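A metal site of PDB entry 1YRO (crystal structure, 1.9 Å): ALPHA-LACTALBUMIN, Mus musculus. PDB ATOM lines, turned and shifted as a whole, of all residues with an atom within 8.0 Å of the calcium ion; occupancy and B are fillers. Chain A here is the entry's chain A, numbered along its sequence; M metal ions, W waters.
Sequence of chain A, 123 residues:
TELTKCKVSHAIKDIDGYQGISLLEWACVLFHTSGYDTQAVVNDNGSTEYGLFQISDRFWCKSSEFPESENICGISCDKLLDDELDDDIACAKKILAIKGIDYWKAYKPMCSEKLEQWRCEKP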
ATOM      1  N   THR A  38      14.333  12.467 -21.707  1.00  0.00           N
ATOM      2  CA  THR A  38      12.938  12.399 -22.129  1.00  0.00           C
ATOM      3  C   THR A  38      12.700  13.044 -23.492  1.00  0.00           C
ATOM      4  O   THR A  38      11.665  12.831 -24.097  1.00  0.00           O
ATOM      5  CB  THR A  38      11.991  13.049 -21.110  1.00  0.00           C
ATOM      6  OG1 THR A  38      12.248  14.457 -21.040  1.00  0.00           O
ATOM      7  CG2 THR A  38      12.197  12.452 -19.718  1.00  0.00           C
ATOM      8  N   ILE A  75      -1.200   7.418 -30.046  1.00  0.00           N
ATOM      9  CA  ILE A  75      -0.693   8.653 -29.466  1.00  0.00           C
ATOM     10  C   ILE A  75       0.233   9.382 -30.414  1.00  0.00           C
ATOM     11  O   ILE A  75       0.882   8.778 -31.255  1.00  0.00           O
ATOM     12  CB  ILE A  75       0.076   8.302 -28.143  1.00  0.00           C
ATOM     13  CG1 ILE A  75       0.446   9.553 -27.379  1.00  0.00           C
ATOM     14  CG2 ILE A  75       1.350   7.542 -28.437  1.00  0.00           C
ATOM     15  CD1 ILE A  75       1.084   9.249 -26.040  1.00  0.00           C
ATOM     16  N   SER A  76       0.282  10.703 -30.275  1.00  0.00           N
ATOM     17  CA  SER A  76       1.185  11.484 -31.091  1.00  0.00           C
ATOM     18  C   SER A  76       2.557  11.236 -30.512  1.00  0.00           C
ATOM     19  O   SER A  76       2.718  11.191 -29.294  1.00  0.00           O
ATOM     20  CB  SER A  76       0.912  12.968 -30.965  1.00  0.00           C
ATOM     21  OG  SER A  76       2.042  13.685 -31.467  1.00  0.00           O
ATOM     22  N   CYS A  77       3.553  11.077 -31.377  1.00  0.00           N
ATOM     23  CA  CYS A  77       4.891  10.851 -30.896  1.00  0.00           C
ATOM     24  C   CYS A  77       5.389  12.041 -30.058  1.00  0.00           C
ATOM     25  O   CYS A  77       6.282  11.879 -29.247  1.00  0.00           O
ATOM     26  CB  CYS A  77       5.837  10.624 -32.066  1.00  0.00           C
ATOM     27  SG  CYS A  77       5.484   9.148 -33.114  1.00  0.00           S
ATOM     28  N   ASP A  78       4.819  13.245 -30.249  1.00  0.00           N
ATOM     29  CA  ASP A  78       5.284  14.388 -29.441  1.00  0.00           C
ATOM     30  C   ASP A  78       4.945  14.267 -27.954  1.00  0.00           C
ATOM     31  O   ASP A  78       5.590  14.923 -27.136  1.00  0.00           O
ATOM     32  CB  ASP A  78       4.715  15.718 -29.962  1.00  0.00           C
ATOM     33  CG  ASP A  78       5.155  16.019 -31.385  1.00  0.00           C
ATOM     34  OD1 ASP A  78       6.334  15.752 -31.714  1.00  0.00           O
ATOM     35  OD2 ASP A  78       4.317  16.525 -32.153  1.00  0.00           O
ATOM     36  N   LYS A  79       3.939  13.454 -27.641  1.00  0.00           N
ATOM     37  CA  LYS A  79       3.558  13.203 -26.248  1.00  0.00           C
ATOM     38  C   LYS A  79       4.647  12.380 -25.546  1.00  0.00           C
ATOM     39  O   LYS A  79       4.629  12.201 -24.313  1.00  0.00           O
ATOM     40  CB  LYS A  79       2.251  12.420 -26.189  1.00  0.00           C
ATOM     41  CG  LYS A  79       1.004  13.217 -26.546  1.00  0.00           C
ATOM     42  CD  LYS A  79       0.679  14.220 -25.431  1.00  0.00           C
ATOM     43  CE  LYS A  79      -0.684  14.909 -25.734  1.00  0.00           C
ATOM     44  NZ  LYS A  79      -1.064  15.844 -24.640  1.00  0.00           N
ATOM     45  N   LEU A  80       5.608  11.917 -26.347  1.00  0.00           N
ATOM     46  CA  LEU A  80       6.691  11.076 -25.833  1.00  0.00           C
ATOM     47  C   LEU A  80       7.970  11.885 -25.646  1.00  0.00           C
ATOM     48  O   LEU A  80       9.042  11.320 -25.357  1.00  0.00           O
ATOM     49  CB  LEU A  80       6.960   9.922 -26.811  1.00  0.00           C
ATOM     50  CG  LEU A  80       5.704   9.093 -27.104  1.00  0.00           C
ATOM     51  CD1 LEU A  80       5.990   7.938 -28.096  1.00  0.00           C
ATOM     52  CD2 LEU A  80       5.194   8.517 -25.794  1.00  0.00           C
ATOM     53  N   LEU A  81       7.841  13.216 -25.787  1.00  0.00           N
ATOM     54  CA  LEU A  81       8.996  14.091 -25.662  1.00  0.00           C
ATOM     55  C   LEU A  81       8.866  15.072 -24.499  1.00  0.00           C
ATOM     56  O   LEU A  81       9.544  16.096 -24.483  1.00  0.00           O
ATOM     57  CB  LEU A  81       9.206  14.859 -26.967  1.00  0.00           C
ATOM     58  CG  LEU A  81       9.508  13.974 -28.207  1.00  0.00           C
ATOM     59  CD1 LEU A  81       9.606  14.826 -29.497  1.00  0.00           C
ATOM     60  CD2 LEU A  81      10.837  13.245 -27.971  1.00  0.00           C
ATOM     61  N   ASP A  82       8.034  14.770 -23.523  1.00  0.00           N
ATOM     62  CA  ASP A  82       7.885  15.681 -22.385  1.00  0.00           C
ATOM     63  C   ASP A  82       8.298  14.951 -21.102  1.00  0.00           C
ATOM     64  O   ASP A  82       8.772  13.811 -21.156  1.00  0.00           O
ATOM     65  CB  ASP A  82       6.430  16.186 -22.306  1.00  0.00           C
ATOM     66  CG  ASP A  82       5.399  15.057 -22.317  1.00  0.00           C
ATOM     67  OD1 ASP A  82       5.569  14.072 -21.574  1.00  0.00           O
ATOM     68  OD2 ASP A  82       4.381  15.156 -23.050  1.00  0.00           O
ATOM     69  N   ASP A  83       8.121  15.600 -19.957  1.00  0.00           N
ATOM     70  CA  ASP A  83       8.524  15.001 -18.684  1.00  0.00           C
ATOM     71  C   ASP A  83       7.441  14.226 -17.947  1.00  0.00           C
ATOM     72  O   ASP A  83       7.636  13.818 -16.810  1.00  0.00           O
ATOM     73  CB  ASP A  83       9.128  16.071 -17.775  1.00  0.00           C
ATOM     74  CG  ASP A  83      10.483  16.562 -18.288  1.00  0.00           C
ATOM     75  OD1 ASP A  83      10.985  15.971 -19.273  1.00  0.00           O
ATOM     76  OD2 ASP A  83      11.052  17.524 -17.711  1.00  0.00           O
ATOM     77  N   GLU A  84       6.315  14.001 -18.604  1.00  0.00           N
ATOM     78  CA  GLU A  84       5.206  13.252 -18.011  1.00  0.00           C
ATOM     79  C   GLU A  84       5.292  11.878 -18.680  1.00  0.00           C
ATOM     80  O   GLU A  84       5.012  11.722 -19.863  1.00  0.00           O
ATOM     81  CB  GLU A  84       3.885  13.975 -18.321  1.00  0.00           C
ATOM     82  CG  GLU A  84       3.782  15.312 -17.545  1.00  0.00           C
ATOM     83  CD  GLU A  84       2.812  16.315 -18.196  1.00  0.00           C
ATOM     84  OE1 GLU A  84       1.636  15.958 -18.380  1.00  0.00           O
ATOM     85  OE2 GLU A  84       3.237  17.438 -18.527  1.00  0.00           O
ATOM     86  N   LEU A  85       5.707  10.894 -17.894  1.00  0.00           N
ATOM     87  CA  LEU A  85       5.943   9.546 -18.381  1.00  0.00           C
ATOM     88  C   LEU A  85       4.791   8.539 -18.383  1.00  0.00           C
ATOM     89  O   LEU A  85       4.965   7.425 -18.881  1.00  0.00           O
ATOM     90  CB  LEU A  85       7.125   8.962 -17.599  1.00  0.00           C
ATOM     91  CG  LEU A  85       8.590   9.262 -17.991  1.00  0.00           C
ATOM     92  CD1 LEU A  85       8.715  10.262 -19.115  1.00  0.00           C
ATOM     93  CD2 LEU A  85       9.350   9.643 -16.779  1.00  0.00           C
ATOM     94  N   ASP A  86       3.636   8.909 -17.848  1.00  0.00           N
ATOM     95  CA  ASP A  86       2.516   7.958 -17.814  1.00  0.00           C
ATOM     96  C   ASP A  86       2.150   7.438 -19.209  1.00  0.00           C
ATOM     97  O   ASP A  86       1.982   6.228 -19.385  1.00  0.00           O
ATOM     98  CB  ASP A  86       1.269   8.571 -17.142  1.00  0.00           C
ATOM     99  CG  ASP A  86       1.466   8.836 -15.651  1.00  0.00           C
ATOM    100  OD1 ASP A  86       2.179   9.795 -15.300  1.00  0.00           O
ATOM    101  OD2 ASP A  86       0.882   8.098 -14.823  1.00  0.00           O
ATOM    102  N   ASP A  87       2.018   8.337 -20.189  1.00  0.00           N
ATOM    103  CA  ASP A  87       1.687   7.842 -21.508  1.00  0.00           C
ATOM    104  C   ASP A  87       2.853   7.064 -22.136  1.00  0.00           C
ATOM    105  O   ASP A  87       2.629   6.028 -22.818  1.00  0.00           O
ATOM    106  CB  ASP A  87       1.176   8.948 -22.453  1.00  0.00           C
ATOM    107  CG  ASP A  87       2.038  10.228 -22.464  1.00  0.00           C
ATOM    108  OD1 ASP A  87       3.173  10.274 -21.920  1.00  0.00           O
ATOM    109  OD2 ASP A  87       1.550  11.212 -23.058  1.00  0.00           O
ATOM    110  N   ASP A  88       4.083   7.521 -21.905  1.00  0.00           N
ATOM    111  CA  ASP A  88       5.252   6.767 -22.446  1.00  0.00           C
ATOM    112  C   ASP A  88       5.218   5.327 -21.892  1.00  0.00           C
ATOM    113  O   ASP A  88       5.397   4.355 -22.637  1.00  0.00           O
ATOM    114  CB  ASP A  88       6.585   7.406 -22.044  1.00  0.00           C
ATOM    115  CG  ASP A  88       6.695   8.851 -22.470  1.00  0.00           C
ATOM    116  OD1 ASP A  88       7.699   9.249 -23.108  1.00  0.00           O
ATOM    117  OD2 ASP A  88       5.737   9.592 -22.158  1.00  0.00           O
ATOM    118  N   ILE A  89       4.978   5.218 -20.588  1.00  0.00           N
ATOM    119  CA  ILE A  89       4.950   3.919 -19.907  1.00  0.00           C
ATOM    120  C   ILE A  89       3.818   3.040 -20.454  1.00  0.00           C
ATOM    121  O   ILE A  89       4.022   1.853 -20.736  1.00  0.00           O
ATOM    122  CB  ILE A  89       4.775   4.143 -18.386  1.00  0.00           C
ATOM    123  CG1 ILE A  89       6.062   4.776 -17.815  1.00  0.00           C
ATOM    124  CG2 ILE A  89       4.477   2.810 -17.673  1.00  0.00           C
ATOM    125  CD1 ILE A  89       5.860   5.373 -16.402  1.00  0.00           C
HETATM  126 CA    CA M   1       4.920  11.816 -22.068  1.00  0.00          CA
HETATM  127  O   HOH W   1       7.197  11.864 -22.580  1.00  0.00           O
HETATM  128  O   HOH W   2       2.873  13.280 -22.067  1.00  0.00           O
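Within 4 Å of the calcium ion: Lys 79, Asp 82, Glu 84, Asp 87 and Asp 88.
Along chain A the residues within 4 Å of the calcium ion span positions 79 to 88.
The nearest printed residue that does not touch the calcium ion is Leu 80 (4.2 Å).
The backbone carbonyl oxygen (O) of Glu 84 binds the calcium ion, 2.2 Å away.
O of Lys 79 is bound to the calcium ion (2.3 Å).
Water W1 is bound to the calcium ion (2.3 Å).
The side-chain carboxylate (OD1) of Asp 87 is bound to the calcium ion (2.3 Å).
OD2 of Asp 88 binds the calcium ion (2.4 Å).
The calcium ion is bound by OD1 of Asp 82 (2.4 Å).
Water W2 binds the calcium ion.
Water W2 bridges OD2 of Asp 82 (2.6 Å) and OD2 of Asp 87 (2.6 Å).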
